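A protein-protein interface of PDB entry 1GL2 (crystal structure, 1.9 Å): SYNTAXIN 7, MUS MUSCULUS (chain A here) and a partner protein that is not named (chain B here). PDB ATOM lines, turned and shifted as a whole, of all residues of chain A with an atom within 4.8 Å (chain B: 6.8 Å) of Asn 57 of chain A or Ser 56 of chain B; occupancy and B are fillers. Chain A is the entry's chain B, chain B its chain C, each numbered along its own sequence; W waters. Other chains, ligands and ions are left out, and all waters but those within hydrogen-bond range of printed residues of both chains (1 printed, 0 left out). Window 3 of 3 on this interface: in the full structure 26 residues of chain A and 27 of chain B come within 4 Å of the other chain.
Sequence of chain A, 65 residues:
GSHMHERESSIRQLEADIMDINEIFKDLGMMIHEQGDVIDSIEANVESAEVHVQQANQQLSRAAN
The side-chain amide oxygen (OD1) of Asn 57 of chain A sits at hydrogen-bond distance from the side-chain hydroxyl (OG) of Ser 56 of chain B (2.6 Å).
The side-chain amide nitrogen (ND2) of Asn 57 of chain A is in hydrogen-bond range of the backbone carbonyl oxygen (O) of Asn 52 of chain B (3.1 Å).
Of the 10 printed residues of chain A, 5 touch a printed residue of chain B.
Among the printed residues, 9 pairs touch across the chains.
Among the printed residues, no Asp or Glu carboxylate lies within 4 Å of a Lys or Arg side-chain nitrogen of the other chain.
Water W1 bridges NZ of Lys 55 of chain B (3.0 Å) and ND2 of Asn 57 of chain A (3.1 Å).
Printed residues of chain B within 4 Å of Val 53 of chain A: Thr 49 (3.5 Å), Asn 52 (3.8 Å) and Leu 53 (3.9 Å).
Of the printed residues of chain B, Gln 54 of chain A touches Asn 52.
Asn 57 of chain A touches three residues of chain B.
Printed residues of chain B within 4 Å of Leu 60 of chain A: Ile 59.
Of the printed residues of chain B, Ser 61 of chain A touches Ile 59 (3.97 Å).
Of chain A, only Asn 57 (2.6 Å) comes within 4 Å of Ser 56 of chain B.
The nearest residue of chain B that does not touch Asn 57 of chain A is Ile 59 of chain B (4.02 Å).
CG2 of Thr 49 of chain B touches CG2 of Val 53 of chain A, at 3.5 Å.
Val 53 of chain A touches Asn 52 of chain B.
Val 53 of chain A touches Leu 53 of chain B.
Asn 52 of chain B touches Gln 54 of chain A.
Asn 57 of chain A touches Lys 55 of chain B.
Ile 59 of chain B touches Leu 60 of chain A (CG2 to O, 3.7 Å).
CG2 of Ile 59 of chain B touches N of Ser 61 of chain A, at 3.97 Å.
The side-chain hydroxyl (OG) of Ser 56 of chain B lies within hydrogen-bond range of the backbone carbonyl oxygen (O) of Asn 52 of chain B.
The side-chain carboxylate (OE2) of Glu 51 of chain B lies within hydrogen-bond range of the side-chain amide nitrogen (ND2) of Asn 52 of chain B.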
ATOM      1  N   VAL A  53      35.948  -4.486  14.811  1.00  0.00           N
ATOM      2  CA  VAL A  53      34.942  -5.541  14.925  1.00  0.00           C
ATOM      3  C   VAL A  53      34.050  -5.199  16.119  1.00  0.00           C
ATOM      4  O   VAL A  53      32.830  -5.350  16.061  1.00  0.00           O
ATOM      5  CB  VAL A  53      35.609  -6.940  15.133  1.00  0.00           C
ATOM      6  CG1 VAL A  53      34.571  -7.978  15.515  1.00  0.00           C
ATOM      7  CG2 VAL A  53      36.313  -7.363  13.861  1.00  0.00           C
ATOM      8  N   GLN A  54      34.670  -4.728  17.198  1.00  0.00           N
ATOM      9  CA  GLN A  54      33.937  -4.338  18.395  1.00  0.00           C
ATOM     10  C   GLN A  54      33.034  -3.145  18.100  1.00  0.00           C
ATOM     11  O   GLN A  54      31.882  -3.116  18.513  1.00  0.00           O
ATOM     12  CB  GLN A  54      34.915  -4.001  19.522  1.00  0.00           C
ATOM     13  CG  GLN A  54      35.555  -5.243  20.132  1.00  0.00           C
ATOM     14  CD  GLN A  54      36.691  -4.925  21.084  1.00  0.00           C
ATOM     15  OE1 GLN A  54      37.084  -5.767  21.895  1.00  0.00           O
ATOM     16  NE2 GLN A  54      37.237  -3.715  20.984  1.00  0.00           N
ATOM     17  N   GLN A  55      33.555  -2.167  17.374  1.00  0.00           N
ATOM     18  CA  GLN A  55      32.766  -0.991  17.016  1.00  0.00           C
ATOM     19  C   GLN A  55      31.632  -1.393  16.076  1.00  0.00           C
ATOM     20  O   GLN A  55      30.510  -0.896  16.193  1.00  0.00           O
ATOM     21  CB  GLN A  55      33.659   0.063  16.352  1.00  0.00           C
ATOM     22  CG  GLN A  55      34.826   0.477  17.231  1.00  0.00           C
ATOM     23  CD  GLN A  55      35.739   1.487  16.580  1.00  0.00           C
ATOM     24  OE1 GLN A  55      36.098   1.359  15.407  1.00  0.00           O
ATOM     25  NE2 GLN A  55      36.140   2.495  17.346  1.00  0.00           N
ATOM     26  N   ALA A  56      31.930  -2.299  15.147  1.00  0.00           N
ATOM     27  CA  ALA A  56      30.938  -2.776  14.191  1.00  0.00           C
ATOM     28  C   ALA A  56      29.789  -3.479  14.910  1.00  0.00           C
ATOM     29  O   ALA A  56      28.624  -3.289  14.560  1.00  0.00           O
ATOM     30  CB  ALA A  56      31.589  -3.725  13.181  1.00  0.00           C
ATOM     31  N   ASN A  57      30.109  -4.295  15.912  1.00  0.00           N
ATOM     32  CA  ASN A  57      29.058  -4.984  16.645  1.00  0.00           C
ATOM     33  C   ASN A  57      28.203  -4.003  17.443  1.00  0.00           C
ATOM     34  O   ASN A  57      27.003  -4.223  17.610  1.00  0.00           O
ATOM     35  CB  ASN A  57      29.638  -6.050  17.578  1.00  0.00           C
ATOM     36  CG  ASN A  57      30.030  -7.314  16.841  1.00  0.00           C
ATOM     37  OD1 ASN A  57      29.566  -7.564  15.728  1.00  0.00           O
ATOM     38  ND2 ASN A  57      30.876  -8.126  17.462  1.00  0.00           N
ATOM     39  N   GLN A  58      28.818  -2.930  17.940  1.00  0.00           N
ATOM     40  CA  GLN A  58      28.077  -1.918  18.691  1.00  0.00           C
ATOM     41  C   GLN A  58      27.002  -1.383  17.756  1.00  0.00           C
ATOM     42  O   GLN A  58      25.839  -1.255  18.134  1.00  0.00           O
ATOM     43  CB  GLN A  58      28.998  -0.774  19.119  1.00  0.00           C
ATOM     44  CG  GLN A  58      30.129  -1.211  20.029  1.00  0.00           C
ATOM     45  CD  GLN A  58      31.199  -0.143  20.224  1.00  0.00           C
ATOM     46  OE1 GLN A  58      32.294  -0.433  20.722  1.00  0.00           O
ATOM     47  NE2 GLN A  58      30.890   1.096  19.841  1.00  0.00           N
ATOM     48  N   GLN A  59      27.409  -1.082  16.528  1.00  0.00           N
ATOM     49  CA  GLN A  59      26.499  -0.576  15.511  1.00  0.00           C
ATOM     50  C   GLN A  59      25.391  -1.568  15.185  1.00  0.00           C
ATOM     51  O   GLN A  59      24.219  -1.220  15.235  1.00  0.00           O
ATOM     52  CB  GLN A  59      27.269  -0.246  14.235  1.00  0.00           C
ATOM     53  CG  GLN A  59      28.176   0.953  14.361  1.00  0.00           C
ATOM     54  CD  GLN A  59      27.415   2.213  14.731  1.00  0.00           C
ATOM     55  OE1 GLN A  59      26.471   2.604  14.042  1.00  0.00           O
ATOM     56  NE2 GLN A  59      27.821   2.854  15.822  1.00  0.00           N
ATOM     57  N   LEU A  60      25.760  -2.799  14.834  1.00  0.00           N
ATOM     58  CA  LEU A  60      24.772  -3.828  14.495  1.00  0.00           C
ATOM     59  C   LEU A  60      23.801  -4.038  15.654  1.00  0.00           C
ATOM     60  O   LEU A  60      22.594  -4.144  15.451  1.00  0.00           O
ATOM     61  CB  LEU A  60      25.465  -5.157  14.151  1.00  0.00           C
ATOM     62  CG  LEU A  60      26.427  -5.150  12.956  1.00  0.00           C
ATOM     63  CD1 LEU A  60      27.065  -6.518  12.808  1.00  0.00           C
ATOM     64  CD2 LEU A  60      25.686  -4.762  11.690  1.00  0.00           C
ATOM     65  N   SER A  61      24.337  -4.087  16.868  1.00  0.00           N
ATOM     66  CA  SER A  61      23.528  -4.275  18.061  1.00  0.00           C
ATOM     67  C   SER A  61      22.513  -3.131  18.229  1.00  0.00           C
ATOM     68  O   SER A  61      21.426  -3.322  18.774  1.00  0.00           O
ATOM     69  CB  SER A  61      24.445  -4.360  19.286  1.00  0.00           C
ATOM     70  OG  SER A  61      23.710  -4.604  20.472  1.00  0.00           O
ATOM     71  N   ARG A  62      22.873  -1.944  17.753  1.00  0.00           N
ATOM     72  CA  ARG A  62      21.990  -0.783  17.844  1.00  0.00           C
ATOM     73  C   ARG A  62      20.911  -0.856  16.762  1.00  0.00           C
ATOM     74  O   ARG A  62      19.776  -0.431  16.974  1.00  0.00           O
ATOM     75  CB  ARG A  62      22.803   0.515  17.700  1.00  0.00           C
ATOM     76  N   THR B  49      38.939 -11.793  18.604  1.00  0.00           N
ATOM     77  CA  THR B  49      38.187 -11.108  17.554  1.00  0.00           C
ATOM     78  C   THR B  49      37.392 -12.110  16.736  1.00  0.00           C
ATOM     79  O   THR B  49      36.260 -11.849  16.329  1.00  0.00           O
ATOM     80  CB  THR B  49      39.125 -10.374  16.598  1.00  0.00           C
ATOM     81  OG1 THR B  49      39.903  -9.424  17.331  1.00  0.00           O
ATOM     82  CG2 THR B  49      38.332  -9.666  15.516  1.00  0.00           C
ATOM     83  N   GLU B  51      36.121 -14.806  17.779  1.00  0.00           N
ATOM     84  CA  GLU B  51      34.940 -15.186  18.546  1.00  0.00           C
ATOM     85  C   GLU B  51      33.918 -14.065  18.527  1.00  0.00           C
ATOM     86  O   GLU B  51      32.720 -14.323  18.590  1.00  0.00           O
ATOM     87  CB  GLU B  51      35.298 -15.521  19.999  1.00  0.00           C
ATOM     88  CG  GLU B  51      34.141 -16.160  20.798  1.00  0.00           C
ATOM     89  CD  GLU B  51      33.198 -15.145  21.448  1.00  0.00           C
ATOM     90  OE1 GLU B  51      32.155 -15.558  22.004  1.00  0.00           O
ATOM     91  OE2 GLU B  51      33.500 -13.933  21.417  1.00  0.00           O
ATOM     92  N   ASN B  52      34.394 -12.823  18.446  1.00  0.00           N
ATOM     93  CA  ASN B  52      33.506 -11.664  18.407  1.00  0.00           C
ATOM     94  C   ASN B  52      32.714 -11.657  17.108  1.00  0.00           C
ATOM     95  O   ASN B  52      31.618 -11.091  17.041  1.00  0.00           O
ATOM     96  CB  ASN B  52      34.305 -10.370  18.515  1.00  0.00           C
ATOM     97  CG  ASN B  52      34.765 -10.087  19.928  1.00  0.00           C
ATOM     98  OD1 ASN B  52      35.540  -9.157  20.165  1.00  0.00           O
ATOM     99  ND2 ASN B  52      34.283 -10.884  20.880  1.00  0.00           N
ATOM    100  N   LEU B  53      33.273 -12.285  16.078  1.00  0.00           N
ATOM    101  CA  LEU B  53      32.602 -12.354  14.790  1.00  0.00           C
ATOM    102  C   LEU B  53      31.446 -13.343  14.851  1.00  0.00           C
ATOM    103  O   LEU B  53      30.540 -13.297  14.016  1.00  0.00           O
ATOM    104  CB  LEU B  53      33.597 -12.730  13.687  1.00  0.00           C
ATOM    105  CG  LEU B  53      34.516 -11.569  13.289  1.00  0.00           C
ATOM    106  CD1 LEU B  53      35.593 -12.059  12.351  1.00  0.00           C
ATOM    107  CD2 LEU B  53      33.694 -10.460  12.634  1.00  0.00           C
ATOM    108  N   SER B  54      31.477 -14.235  15.840  1.00  0.00           N
ATOM    109  CA  SER B  54      30.393 -15.199  16.016  1.00  0.00           C
ATOM    110  C   SER B  54      29.203 -14.441  16.592  1.00  0.00           C
ATOM    111  O   SER B  54      28.055 -14.772  16.312  1.00  0.00           O
ATOM    112  CB  SER B  54      30.800 -16.336  16.962  1.00  0.00           C
ATOM    113  OG  SER B  54      31.657 -17.262  16.311  1.00  0.00           O
ATOM    114  N   LYS B  55      29.480 -13.423  17.402  1.00  0.00           N
ATOM    115  CA  LYS B  55      28.412 -12.613  17.965  1.00  0.00           C
ATOM    116  C   LYS B  55      27.827 -11.748  16.844  1.00  0.00           C
ATOM    117  O   LYS B  55      26.633 -11.448  16.838  1.00  0.00           O
ATOM    118  CB  LYS B  55      28.933 -11.724  19.096  1.00  0.00           C
ATOM    119  CG  LYS B  55      27.888 -10.723  19.600  1.00  0.00           C
ATOM    120  CD  LYS B  55      28.267 -10.105  20.931  1.00  0.00           C
ATOM    121  CE  LYS B  55      29.573  -9.347  20.846  1.00  0.00           C
ATOM    122  NZ  LYS B  55      29.980  -8.826  22.184  1.00  0.00           N
ATOM    123  N   SER B  56      28.673 -11.348  15.896  1.00  0.00           N
ATOM    124  CA  SER B  56      28.224 -10.548  14.758  1.00  0.00           C
ATOM    125  C   SER B  56      27.141 -11.360  14.047  1.00  0.00           C
ATOM    126  O   SER B  56      26.050 -10.862  13.752  1.00  0.00           O
ATOM    127  CB  SER B  56      29.378 -10.300  13.773  1.00  0.00           C
ATOM    128  OG  SER B  56      30.468  -9.614  14.366  1.00  0.00           O
ATOM    129  N   ARG B  57      27.474 -12.622  13.774  1.00  0.00           N
ATOM    130  CA  ARG B  57      26.588 -13.559  13.096  1.00  0.00           C
ATOM    131  C   ARG B  57      25.265 -13.694  13.845  1.00  0.00           C
ATOM    132  O   ARG B  57      24.195 -13.699  13.236  1.00  0.00           O
ATOM    133  CB  ARG B  57      27.285 -14.924  12.986  1.00  0.00           C
ATOM    134  CG  ARG B  57      26.492 -15.993  12.258  1.00  0.00           C
ATOM    135  CD  ARG B  57      27.362 -17.218  11.975  1.00  0.00           C
ATOM    136  NE  ARG B  57      26.605 -18.275  11.308  1.00  0.00           N
ATOM    137  CZ  ARG B  57      25.707 -19.048  11.913  1.00  0.00           C
ATOM    138  NH1 ARG B  57      25.453 -18.893  13.208  1.00  0.00           N
ATOM    139  NH2 ARG B  57      25.047 -19.968  11.221  1.00  0.00           N
ATOM    140  N   LYS B  58      25.351 -13.799  15.168  1.00  0.00           N
ATOM    141  CA  LYS B  58      24.172 -13.931  16.007  1.00  0.00           C
ATOM    142  C   LYS B  58      23.266 -12.705  15.880  1.00  0.00           C
ATOM    143  O   LYS B  58      22.049 -12.830  15.705  1.00  0.00           O
ATOM    144  CB  LYS B  58      24.591 -14.115  17.465  1.00  0.00           C
ATOM    145  CG  LYS B  58      23.432 -14.335  18.414  1.00  0.00           C
ATOM    146  CD  LYS B  58      23.914 -14.518  19.835  1.00  0.00           C
ATOM    147  CE  LYS B  58      22.747 -14.751  20.777  1.00  0.00           C
ATOM    148  NZ  LYS B  58      23.210 -14.882  22.189  1.00  0.00           N
ATOM    149  N   ILE B  59      23.863 -11.520  15.966  1.00  0.00           N
ATOM    150  CA  ILE B  59      23.106 -10.277  15.852  1.00  0.00           C
ATOM    151  C   ILE B  59      22.462 -10.156  14.473  1.00  0.00           C
ATOM    152  O   ILE B  59      21.310  -9.736  14.346  1.00  0.00           O
ATOM    153  CB  ILE B  59      24.008  -9.033  16.072  1.00  0.00           C
ATOM    154  CG1 ILE B  59      24.656  -9.086  17.460  1.00  0.00           C
ATOM    155  CG2 ILE B  59      23.175  -7.762  15.925  1.00  0.00           C
ATOM    156  CD1 ILE B  59      25.727  -8.038  17.685  1.00  0.00           C
ATOM    157  N   LEU B  60      23.212 -10.515  13.436  1.00  0.00           N
ATOM    158  CA  LEU B  60      22.693 -10.431  12.078  1.00  0.00           C
ATOM    159  C   LEU B  60      21.561 -11.434  11.868  1.00  0.00           C
ATOM    160  O   LEU B  60      20.627 -11.177  11.109  1.00  0.00           O
ATOM    161  CB  LEU B  60      23.823 -10.650  11.061  1.00  0.00           C
ATOM    162  CG  LEU B  60      24.813  -9.477  10.952  1.00  0.00           C
ATOM    163  CD1 LEU B  60      26.015  -9.859  10.098  1.00  0.00           C
ATOM    164  CD2 LEU B  60      24.099  -8.270  10.359  1.00  0.00           C
ATOM    165  N   ARG B  61      21.639 -12.573  12.549  1.00  0.00           N
ATOM    166  CA  ARG B  61      20.595 -13.581  12.429  1.00  0.00           C
ATOM    167  C   ARG B  61      19.277 -13.040  12.968  1.00  0.00           C
ATOM    168  O   ARG B  61      18.218 -13.297  12.402  1.00  0.00           O
ATOM    169  CB  ARG B  61      20.987 -14.854  13.181  1.00  0.00           C
ATOM    170  CG  ARG B  61      21.927 -15.767  12.403  1.00  0.00           C
ATOM    171  CD  ARG B  61      22.356 -16.954  13.248  1.00  0.00           C
ATOM    172  NE  ARG B  61      21.214 -17.656  13.840  1.00  0.00           N
ATOM    173  CZ  ARG B  61      20.424 -18.504  13.187  1.00  0.00           C
ATOM    174  NH1 ARG B  61      20.639 -18.773  11.907  1.00  0.00           N
ATOM    175  NH2 ARG B  61      19.423 -19.099  13.820  1.00  0.00           N
HETATM  176  O   HOH W   1      31.893  -7.413  20.304  1.00  0.00           O
